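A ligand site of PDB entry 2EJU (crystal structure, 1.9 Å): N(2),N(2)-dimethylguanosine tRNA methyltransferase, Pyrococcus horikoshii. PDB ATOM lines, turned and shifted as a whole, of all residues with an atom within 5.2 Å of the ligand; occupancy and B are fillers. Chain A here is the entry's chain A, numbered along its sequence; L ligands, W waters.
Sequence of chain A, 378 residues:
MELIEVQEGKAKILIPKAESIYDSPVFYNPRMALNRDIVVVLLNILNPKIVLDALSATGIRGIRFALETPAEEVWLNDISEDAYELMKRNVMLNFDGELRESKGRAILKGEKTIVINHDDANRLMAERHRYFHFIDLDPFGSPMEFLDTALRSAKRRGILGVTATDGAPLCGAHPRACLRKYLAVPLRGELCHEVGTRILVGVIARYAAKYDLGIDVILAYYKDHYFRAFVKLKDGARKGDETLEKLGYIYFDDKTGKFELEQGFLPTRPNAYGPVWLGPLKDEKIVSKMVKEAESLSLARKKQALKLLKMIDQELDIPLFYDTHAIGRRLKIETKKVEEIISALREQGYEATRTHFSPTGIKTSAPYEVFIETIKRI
Water W4 lies within hydrogen-bond range of O4 of the ligand (2.7 Å) and N of Phe 27 (2.8 Å). Water W3 lies within hydrogen-bond range of the backbone carbonyl oxygen of Phe 27 (2.8 Å), an oxygen (O1) of the ligand (2.8 Å) and the side-chain hydroxyl of Thr 58 (2.8 Å). Water W8 bridges the guanidinium group of Arg 36 (2.9 Å) and an oxygen (O1) of the ligand (2.9 Å). Water W5 lies within hydrogen-bond range of N4 of the ligand (2.9 Å) and OE2 of Glu 145 (3.0 Å). Water W1 lies within hydrogen-bond range of the backbone NH (N) of Phe 140 (2.7 Å) and an oxygen (O3) of the ligand (3.2 Å). Water W7 lies within hydrogen-bond range of the backbone carbonyl oxygen of Ser 56 (2.6 Å), the backbone NH of Arg 61 (2.9 Å), the side-chain carboxylate of Asp 53 (3.0 Å) and the backbone NH of Ile 60 (3.5 Å).
The backbone carbonyl oxygen of Leu 55 lies within hydrogen-bond range of a nitrogen (N1) of the ligand (2.6 Å). N6 of the ligand lies within hydrogen-bond range of N of Ile 79, at 3.4 Å. NH1 of Arg 61 is in salt-bridge range of O2 of the ligand (3.0 Å). The backbone NH of Ala 121 is in hydrogen-bond range of a nitrogen (N5) of the ligand, 2.7 Å away. The side-chain carboxylate (OD2) of Asp 138 is in salt-bridge range of a nitrogen (N1) of the ligand (3.0 Å). The guanidinium group (NH1) of Arg 36 lies within salt-bridge range of an oxygen (O2) of the ligand. The side-chain carboxylate of Asp 120 sits at hydrogen-bond distance from a nitrogen (N4) of the ligand, 2.8 Å away. O4 of the ligand sits at hydrogen-bond distance from OD1 of Asp 78, 2.5 Å away.
Merely in contact with the ligand: Ala 57, Phe 146, Phe 140, Ile 60, Asp 119, Asn 77, Ser 80, Phe 27 and Ala 54. 17 residues have an atom within 4 Å of the ligand: Phe 27, Arg 36, Ala 54, Leu 55, Ala 57, Ile 60, Arg 61, Asn 77, Asp 78, Ile 79, Ser 80, Asp 119, Asp 120, Ala 121, Asp 138, Phe 140 and Phe 146.
O of Asn 77 lies within hydrogen-bond range of OG of Ser 56 (2.9 Å). N of Ala 83 is in hydrogen-bond range of OG of Ser 80, 3.3 Å away. N of Asn 77 lies within hydrogen-bond range of O of Asp 53, at 3.0 Å. N of Ser 80 sits at hydrogen-bond distance from OD2 of Asp 78 (3.0 Å). The backbone NH (N) of Ala 57 lies within hydrogen-bond range of the side-chain carboxylate (OD1) of Asp 78, 2.8 Å away. The backbone NH (N) of Ile 79 sits at hydrogen-bond distance from the backbone carbonyl oxygen (O) of Asp 119 (3.2 Å). OD1 of Asp 120 is in hydrogen-bond range of N of Asn 122, at 3.0 Å. The side-chain carboxylate (OD2) of Asp 138 lies within salt-bridge range of the guanidinium group (NH1) of Arg 61 (3.0 Å).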
ATOM      1  N   PHE A  27      21.265 -12.095 -19.367  1.00  0.00           N
ATOM      2  CA  PHE A  27      21.504 -12.238 -17.939  1.00  0.00           C
ATOM      3  C   PHE A  27      22.460 -11.245 -17.278  1.00  0.00           C
ATOM      4  O   PHE A  27      23.527 -10.923 -17.811  1.00  0.00           O
ATOM      5  CB  PHE A  27      21.962 -13.667 -17.647  1.00  0.00           C
ATOM      6  CG  PHE A  27      22.153 -13.965 -16.192  1.00  0.00           C
ATOM      7  CD1 PHE A  27      23.383 -13.780 -15.572  1.00  0.00           C
ATOM      8  CD2 PHE A  27      21.085 -14.437 -15.430  1.00  0.00           C
ATOM      9  CE1 PHE A  27      23.565 -14.074 -14.226  1.00  0.00           C
ATOM     10  CE2 PHE A  27      21.253 -14.727 -14.065  1.00  0.00           C
ATOM     11  CZ  PHE A  27      22.496 -14.540 -13.472  1.00  0.00           C
ATOM     12  N   TYR A  28      22.052 -10.775 -16.102  1.00  0.00           N
ATOM     13  CA  TYR A  28      22.848  -9.870 -15.293  1.00  0.00           C
ATOM     14  C   TYR A  28      22.480 -10.064 -13.832  1.00  0.00           C
ATOM     15  O   TYR A  28      21.302  -9.984 -13.469  1.00  0.00           O
ATOM     16  CB  TYR A  28      22.607  -8.404 -15.654  1.00  0.00           C
ATOM     17  CG  TYR A  28      23.364  -7.476 -14.731  1.00  0.00           C
ATOM     18  CD1 TYR A  28      24.761  -7.429 -14.754  1.00  0.00           C
ATOM     19  CD2 TYR A  28      22.698  -6.699 -13.787  1.00  0.00           C
ATOM     20  CE1 TYR A  28      25.470  -6.630 -13.859  1.00  0.00           C
ATOM     21  CE2 TYR A  28      23.387  -5.897 -12.887  1.00  0.00           C
ATOM     22  CZ  TYR A  28      24.776  -5.874 -12.926  1.00  0.00           C
ATOM     23  OH  TYR A  28      25.481  -5.103 -12.027  1.00  0.00           O
ATOM     24  N   ARG A  36      33.068  -9.769  -9.590  1.00  0.00           N
ATOM     25  CA  ARG A  36      33.712  -8.907 -10.582  1.00  0.00           C
ATOM     26  C   ARG A  36      34.788  -8.035  -9.919  1.00  0.00           C
ATOM     27  O   ARG A  36      35.881  -7.875 -10.453  1.00  0.00           O
ATOM     28  CB  ARG A  36      32.673  -8.014 -11.268  1.00  0.00           C
ATOM     29  CG  ARG A  36      32.479  -8.276 -12.760  1.00  0.00           C
ATOM     30  CD  ARG A  36      31.148  -8.966 -13.051  1.00  0.00           C
ATOM     31  NE  ARG A  36      29.996  -8.251 -12.497  1.00  0.00           N
ATOM     32  CZ  ARG A  36      28.761  -8.734 -12.480  1.00  0.00           C
ATOM     33  NH1 ARG A  36      28.501  -9.920 -13.018  1.00  0.00           N
ATOM     34  NH2 ARG A  36      27.778  -8.062 -11.896  1.00  0.00           N
ATOM     35  N   ASP A  53      36.881 -12.369 -21.664  1.00  0.00           N
ATOM     36  CA  ASP A  53      35.667 -12.494 -20.868  1.00  0.00           C
ATOM     37  C   ASP A  53      34.876 -13.414 -21.803  1.00  0.00           C
ATOM     38  O   ASP A  53      34.160 -12.952 -22.707  1.00  0.00           O
ATOM     39  CB  ASP A  53      35.002 -11.132 -20.694  1.00  0.00           C
ATOM     40  CG  ASP A  53      33.649 -11.224 -20.002  1.00  0.00           C
ATOM     41  OD1 ASP A  53      33.307 -12.307 -19.495  1.00  0.00           O
ATOM     42  OD2 ASP A  53      32.941 -10.194 -19.949  1.00  0.00           O
ATOM     43  N   ALA A  54      35.025 -14.729 -21.591  1.00  0.00           N
ATOM     44  CA  ALA A  54      34.430 -15.770 -22.435  1.00  0.00           C
ATOM     45  C   ALA A  54      32.909 -15.890 -22.552  1.00  0.00           C
ATOM     46  O   ALA A  54      32.408 -16.298 -23.598  1.00  0.00           O
ATOM     47  CB  ALA A  54      35.020 -17.118 -22.053  1.00  0.00           C
ATOM     48  N   LEU A  55      32.194 -15.579 -21.487  1.00  0.00           N
ATOM     49  CA  LEU A  55      30.722 -15.638 -21.500  1.00  0.00           C
ATOM     50  C   LEU A  55      30.333 -14.346 -20.790  1.00  0.00           C
ATOM     51  O   LEU A  55      30.025 -14.346 -19.596  1.00  0.00           O
ATOM     52  CB  LEU A  55      30.239 -16.879 -20.737  1.00  0.00           C
ATOM     53  CG  LEU A  55      30.899 -18.185 -21.185  1.00  0.00           C
ATOM     54  CD1 LEU A  55      31.926 -18.591 -20.136  1.00  0.00           C
ATOM     55  CD2 LEU A  55      29.874 -19.290 -21.349  1.00  0.00           C
ATOM     56  N   SER A  56      30.358 -13.247 -21.538  1.00  0.00           N
ATOM     57  CA  SER A  56      30.096 -11.924 -20.989  1.00  0.00           C
ATOM     58  C   SER A  56      28.668 -11.430 -20.813  1.00  0.00           C
ATOM     59  O   SER A  56      28.445 -10.475 -20.070  1.00  0.00           O
ATOM     60  CB  SER A  56      30.888 -10.891 -21.809  1.00  0.00           C
ATOM     61  OG  SER A  56      30.885 -11.233 -23.177  1.00  0.00           O
ATOM     62  N   ALA A  57      27.702 -12.056 -21.483  1.00  0.00           N
ATOM     63  CA  ALA A  57      26.307 -11.622 -21.347  1.00  0.00           C
ATOM     64  C   ALA A  57      26.127 -10.144 -21.720  1.00  0.00           C
ATOM     65  O   ALA A  57      26.124  -9.798 -22.904  1.00  0.00           O
ATOM     66  CB  ALA A  57      25.826 -11.867 -19.920  1.00  0.00           C
ATOM     67  N   THR A  58      25.982  -9.285 -20.720  1.00  0.00           N
ATOM     68  CA  THR A  58      25.814  -7.861 -20.985  1.00  0.00           C
ATOM     69  C   THR A  58      27.157  -7.210 -21.310  1.00  0.00           C
ATOM     70  O   THR A  58      27.207  -6.097 -21.823  1.00  0.00           O
ATOM     71  CB  THR A  58      25.231  -7.106 -19.766  1.00  0.00           C
ATOM     72  OG1 THR A  58      26.166  -7.144 -18.686  1.00  0.00           O
ATOM     73  CG2 THR A  58      23.912  -7.747 -19.323  1.00  0.00           C
ATOM     74  N   ILE A  60      29.478  -6.612 -18.959  1.00  0.00           N
ATOM     75  CA  ILE A  60      29.961  -5.885 -17.779  1.00  0.00           C
ATOM     76  C   ILE A  60      31.366  -6.250 -17.317  1.00  0.00           C
ATOM     77  O   ILE A  60      32.155  -5.370 -16.971  1.00  0.00           O
ATOM     78  CB  ILE A  60      28.980  -6.048 -16.578  1.00  0.00           C
ATOM     79  CG1 ILE A  60      29.509  -5.285 -15.365  1.00  0.00           C
ATOM     80  CG2 ILE A  60      28.819  -7.522 -16.223  1.00  0.00           C
ATOM     81  CD1 ILE A  60      29.703  -3.803 -15.605  1.00  0.00           C
ATOM     82  N   ARG A  61      31.693  -7.545 -17.309  1.00  0.00           N
ATOM     83  CA  ARG A  61      33.009  -7.982 -16.864  1.00  0.00           C
ATOM     84  C   ARG A  61      34.133  -7.427 -17.735  1.00  0.00           C
ATOM     85  O   ARG A  61      35.009  -6.719 -17.243  1.00  0.00           O
ATOM     86  CB  ARG A  61      33.063  -9.518 -16.832  1.00  0.00           C
ATOM     87  CG  ARG A  61      34.213 -10.089 -16.043  1.00  0.00           C
ATOM     88  CD  ARG A  61      34.086 -11.617 -15.951  1.00  0.00           C
ATOM     89  NE  ARG A  61      32.918 -12.011 -15.177  1.00  0.00           N
ATOM     90  CZ  ARG A  61      32.952 -12.433 -13.918  1.00  0.00           C
ATOM     91  NH1 ARG A  61      31.825 -12.756 -13.300  1.00  0.00           N
ATOM     92  NH2 ARG A  61      34.110 -12.546 -13.275  1.00  0.00           N
ATOM     93  N   ASN A  77      32.904 -12.096 -25.280  1.00  0.00           N
ATOM     94  CA  ASN A  77      32.247 -13.085 -26.113  1.00  0.00           C
ATOM     95  C   ASN A  77      30.984 -13.680 -25.530  1.00  0.00           C
ATOM     96  O   ASN A  77      30.865 -13.849 -24.318  1.00  0.00           O
ATOM     97  CB  ASN A  77      33.222 -14.230 -26.423  1.00  0.00           C
ATOM     98  CG  ASN A  77      32.580 -15.308 -27.263  1.00  0.00           C
ATOM     99  OD1 ASN A  77      32.481 -15.188 -28.477  1.00  0.00           O
ATOM    100  ND2 ASN A  77      32.127 -16.374 -26.599  1.00  0.00           N
ATOM    101  N   ASP A  78      30.049 -14.019 -26.403  1.00  0.00           N
ATOM    102  CA  ASP A  78      28.803 -14.660 -25.997  1.00  0.00           C
ATOM    103  C   ASP A  78      28.166 -15.290 -27.218  1.00  0.00           C
ATOM    104  O   ASP A  78      28.235 -14.759 -28.321  1.00  0.00           O
ATOM    105  CB  ASP A  78      27.845 -13.650 -25.361  1.00  0.00           C
ATOM    106  CG  ASP A  78      26.860 -14.317 -24.420  1.00  0.00           C
ATOM    107  OD1 ASP A  78      26.964 -14.090 -23.194  1.00  0.00           O
ATOM    108  OD2 ASP A  78      25.981 -15.072 -24.897  1.00  0.00           O
ATOM    109  N   ILE A  79      27.528 -16.443 -27.023  1.00  0.00           N
ATOM    110  CA  ILE A  79      26.905 -17.140 -28.120  1.00  0.00           C
ATOM    111  C   ILE A  79      25.538 -16.543 -28.498  1.00  0.00           C
ATOM    112  O   ILE A  79      25.061 -16.727 -29.618  1.00  0.00           O
ATOM    113  CB  ILE A  79      26.732 -18.640 -27.757  1.00  0.00           C
ATOM    114  CG1 ILE A  79      26.432 -19.465 -29.016  1.00  0.00           C
ATOM    115  CG2 ILE A  79      25.615 -18.804 -26.739  1.00  0.00           C
ATOM    116  CD1 ILE A  79      26.307 -20.950 -28.751  1.00  0.00           C
ATOM    117  N   SER A  80      24.923 -15.830 -27.560  1.00  0.00           N
ATOM    118  CA  SER A  80      23.615 -15.238 -27.798  1.00  0.00           C
ATOM    119  C   SER A  80      23.631 -13.953 -28.606  1.00  0.00           C
ATOM    120  O   SER A  80      24.401 -13.029 -28.312  1.00  0.00           O
ATOM    121  CB  SER A  80      22.929 -14.970 -26.453  1.00  0.00           C
ATOM    122  OG  SER A  80      21.792 -14.139 -26.626  1.00  0.00           O
ATOM    123  N   ALA A  83      22.707 -11.006 -26.475  1.00  0.00           N
ATOM    124  CA  ALA A  83      23.815 -10.597 -25.626  1.00  0.00           C
ATOM    125  C   ALA A  83      24.828  -9.813 -26.457  1.00  0.00           C
ATOM    126  O   ALA A  83      25.298  -8.763 -26.031  1.00  0.00           O
ATOM    127  CB  ALA A  83      24.485 -11.825 -24.986  1.00  0.00           C
ATOM    128  N   ASP A 119      29.781 -15.787 -30.641  1.00  0.00           N
ATOM    129  CA  ASP A 119      30.080 -17.167 -30.986  1.00  0.00           C
ATOM    130  C   ASP A 119      30.180 -18.068 -29.750  1.00  0.00           C
ATOM    131  O   ASP A 119      30.095 -17.605 -28.618  1.00  0.00           O
ATOM    132  CB  ASP A 119      31.416 -17.219 -31.735  1.00  0.00           C
ATOM    133  CG  ASP A 119      31.581 -18.462 -32.601  1.00  0.00           C
ATOM    134  OD1 ASP A 119      32.618 -18.550 -33.279  1.00  0.00           O
ATOM    135  OD2 ASP A 119      30.692 -19.344 -32.590  1.00  0.00           O
ATOM    136  N   ASP A 120      30.350 -19.368 -30.000  1.00  0.00           N
ATOM    137  CA  ASP A 120      30.522 -20.358 -28.945  1.00  0.00           C
ATOM    138  C   ASP A 120      31.902 -20.061 -28.377  1.00  0.00           C
ATOM    139  O   ASP A 120      32.871 -19.888 -29.137  1.00  0.00           O
ATOM    140  CB  ASP A 120      30.533 -21.765 -29.557  1.00  0.00           C
ATOM    141  CG  ASP A 120      30.666 -22.867 -28.505  1.00  0.00           C
ATOM    142  OD1 ASP A 120      31.032 -22.579 -27.351  1.00  0.00           O
ATOM    143  OD2 ASP A 120      30.408 -24.030 -28.861  1.00  0.00           O
ATOM    144  N   ALA A 121      31.998 -19.989 -27.054  1.00  0.00           N
ATOM    145  CA  ALA A 121      33.270 -19.711 -26.408  1.00  0.00           C
ATOM    146  C   ALA A 121      34.337 -20.727 -26.800  1.00  0.00           C
ATOM    147  O   ALA A 121      35.506 -20.374 -26.944  1.00  0.00           O
ATOM    148  CB  ALA A 121      33.097 -19.693 -24.893  1.00  0.00           C
ATOM    149  N   ASN A 122      33.930 -21.992 -26.956  1.00  0.00           N
ATOM    150  CA  ASN A 122      34.879 -23.038 -27.339  1.00  0.00           C
ATOM    151  C   ASN A 122      35.446 -22.774 -28.727  1.00  0.00           C
ATOM    152  O   ASN A 122      36.617 -23.055 -29.002  1.00  0.00           O
ATOM    153  CB  ASN A 122      34.227 -24.428 -27.324  1.00  0.00           C
ATOM    154  CG  ASN A 122      34.277 -25.072 -25.958  1.00  0.00           C
ATOM    155  OD1 ASN A 122      35.269 -24.955 -25.251  1.00  0.00           O
ATOM    156  ND2 ASN A 122      33.204 -25.766 -25.582  1.00  0.00           N
ATOM    157  N   ASP A 138      33.078 -17.620 -16.688  1.00  0.00           N
ATOM    158  CA  ASP A 138      31.977 -17.396 -15.756  1.00  0.00           C
ATOM    159  C   ASP A 138      30.666 -17.812 -16.425  1.00  0.00           C
ATOM    160  O   ASP A 138      29.897 -16.971 -16.902  1.00  0.00           O
ATOM    161  CB  ASP A 138      31.924 -15.914 -15.372  1.00  0.00           C
ATOM    162  CG  ASP A 138      30.981 -15.652 -14.232  1.00  0.00           C
ATOM    163  OD1 ASP A 138      31.199 -16.215 -13.136  1.00  0.00           O
ATOM    164  OD2 ASP A 138      30.015 -14.888 -14.432  1.00  0.00           O
ATOM    165  N   PRO A 139      30.382 -19.119 -16.456  1.00  0.00           N
ATOM    166  CA  PRO A 139      29.165 -19.650 -17.064  1.00  0.00           C
ATOM    167  C   PRO A 139      27.978 -19.784 -16.125  1.00  0.00           C
ATOM    168  O   PRO A 139      28.054 -19.452 -14.942  1.00  0.00           O
ATOM    169  CB  PRO A 139      29.614 -21.013 -17.559  1.00  0.00           C
ATOM    170  CG  PRO A 139      30.453 -21.468 -16.403  1.00  0.00           C
ATOM    171  CD  PRO A 139      31.283 -20.221 -16.074  1.00  0.00           C
ATOM    172  N   PHE A 140      26.875 -20.269 -16.691  1.00  0.00           N
ATOM    173  CA  PHE A 140      25.647 -20.538 -15.938  1.00  0.00           C
ATOM    174  C   PHE A 140      25.861 -21.938 -15.370  1.00  0.00           C
ATOM    175  O   PHE A 140      25.539 -22.919 -16.021  1.00  0.00           O
ATOM    176  CB  PHE A 140      24.432 -20.630 -16.857  1.00  0.00           C
ATOM    177  CG  PHE A 140      23.825 -19.309 -17.246  1.00  0.00           C
ATOM    178  CD1 PHE A 140      23.653 -18.307 -16.308  1.00  0.00           C
ATOM    179  CD2 PHE A 140      23.347 -19.112 -18.543  1.00  0.00           C
ATOM    180  CE1 PHE A 140      23.008 -17.125 -16.645  1.00  0.00           C
ATOM    181  CE2 PHE A 140      22.698 -17.931 -18.892  1.00  0.00           C
ATOM    182  CZ  PHE A 140      22.528 -16.935 -17.947  1.00  0.00           C
ATOM    183  N   GLU A 145      32.475 -27.562 -19.664  1.00  0.00           N
ATOM    184  CA  GLU A 145      32.348 -27.653 -21.125  1.00  0.00           C
ATOM    185  C   GLU A 145      33.399 -26.781 -21.830  1.00  0.00           C
ATOM    186  O   GLU A 145      33.703 -26.992 -22.994  1.00  0.00           O
ATOM    187  CB  GLU A 145      30.953 -27.192 -21.565  1.00  0.00           C
ATOM    188  CG  GLU A 145      30.727 -27.288 -23.077  1.00  0.00           C
ATOM    189  CD  GLU A 145      29.379 -26.725 -23.522  1.00  0.00           C
ATOM    190  OE1 GLU A 145      28.509 -26.509 -22.658  1.00  0.00           O
ATOM    191  OE2 GLU A 145      29.188 -26.503 -24.745  1.00  0.00           O
ATOM    192  N   PHE A 146      33.944 -25.816 -21.087  1.00  0.00           N
ATOM    193  CA  PHE A 146      34.909 -24.875 -21.650  1.00  0.00           C
ATOM    194  C   PHE A 146      36.341 -24.973 -21.128  1.00  0.00           C
ATOM    195  O   PHE A 146      37.249 -24.374 -21.702  1.00  0.00           O
ATOM    196  CB  PHE A 146      34.382 -23.456 -21.391  1.00  0.00           C
ATOM    197  CG  PHE A 146      32.931 -23.280 -21.762  1.00  0.00           C
ATOM    198  CD1 PHE A 146      32.540 -23.264 -23.098  1.00  0.00           C
ATOM    199  CD2 PHE A 146      31.952 -23.176 -20.776  1.00  0.00           C
ATOM    200  CE1 PHE A 146      31.199 -23.149 -23.456  1.00  0.00           C
ATOM    201  CE2 PHE A 146      30.606 -23.064 -21.110  1.00  0.00           C
ATOM    202  CZ  PHE A 146      30.225 -23.050 -22.449  1.00  0.00           C
HETATM  203  N1  LIG L   1      30.049 -13.440 -17.112  1.00  0.00           N
HETATM  204  C1  LIG L   1      29.075 -12.724 -16.522  1.00  0.00           C
HETATM  205  C2  LIG L   1      27.890 -13.634 -16.917  1.00  0.00           C
HETATM  206  C3  LIG L   1      27.302 -14.819 -17.581  1.00  0.00           C
HETATM  207  S1  LIG L   1      25.804 -15.590 -17.819  1.00  0.00           S
HETATM  208  C4  LIG L   1      29.001 -11.536 -15.750  1.00  0.00           C
HETATM  209  O1  LIG L   1      27.875 -10.914 -15.995  1.00  0.00           O
HETATM  210  O2  LIG L   1      29.928 -11.213 -14.977  1.00  0.00           O
HETATM  211  C5  LIG L   1      26.329 -16.896 -18.791  1.00  0.00           C
HETATM  212  C6  LIG L   1      25.733 -16.737 -20.227  1.00  0.00           C
HETATM  213  O3  LIG L   1      26.575 -17.635 -20.962  1.00  0.00           O
HETATM  214  C7  LIG L   1      24.909 -15.972 -21.235  1.00  0.00           C
HETATM  215  O4  LIG L   1      25.035 -14.568 -21.601  1.00  0.00           O
HETATM  216  C8  LIG L   1      24.971 -16.835 -22.493  1.00  0.00           C
HETATM  217  O5  LIG L   1      24.248 -16.758 -23.589  1.00  0.00           O
HETATM  218  C9  LIG L   1      26.034 -17.869 -22.249  1.00  0.00           C
HETATM  219  N2  LIG L   1      26.616 -19.077 -23.066  1.00  0.00           N
HETATM  220  C10 LIG L   1      26.083 -20.282 -22.992  1.00  0.00           C
HETATM  221  N3  LIG L   1      26.740 -21.107 -23.756  1.00  0.00           N
HETATM  222  C11 LIG L   1      27.721 -20.464 -24.321  1.00  0.00           C
HETATM  223  C12 LIG L   1      28.737 -20.837 -25.215  1.00  0.00           C
HETATM  224  N4  LIG L   1      28.813 -22.097 -25.635  1.00  0.00           N
HETATM  225  N5  LIG L   1      29.671 -19.889 -25.665  1.00  0.00           N
HETATM  226  C13 LIG L   1      29.615 -18.573 -25.243  1.00  0.00           C
HETATM  227  N6  LIG L   1      28.628 -18.184 -24.367  1.00  0.00           N
HETATM  228  C14 LIG L   1      27.662 -19.117 -23.887  1.00  0.00           C
HETATM  229  O   HOH W   1      27.098 -20.345 -19.351  1.00  0.00           O
HETATM  230  O   HOH W   2      22.307 -18.424 -24.431  1.00  0.00           O
HETATM  231  O   HOH W   3      25.950  -9.643 -17.508  1.00  0.00           O
HETATM  232  O   HOH W   4      22.500 -13.618 -21.356  1.00  0.00           O
HETATM  233  O   HOH W   5      27.135 -24.431 -25.202  1.00  0.00           O
HETATM  234  O   HOH W   6      23.810 -22.386 -24.562  1.00  0.00           O
HETATM  235  O   HOH W   7      30.384  -9.893 -18.369  1.00  0.00           O
HETATM  236  O   HOH W   8      26.047 -11.263 -13.772  1.00  0.00           O
HETATM  237  O   HOH W   9      26.073 -23.742 -22.953  1.00  0.00           O
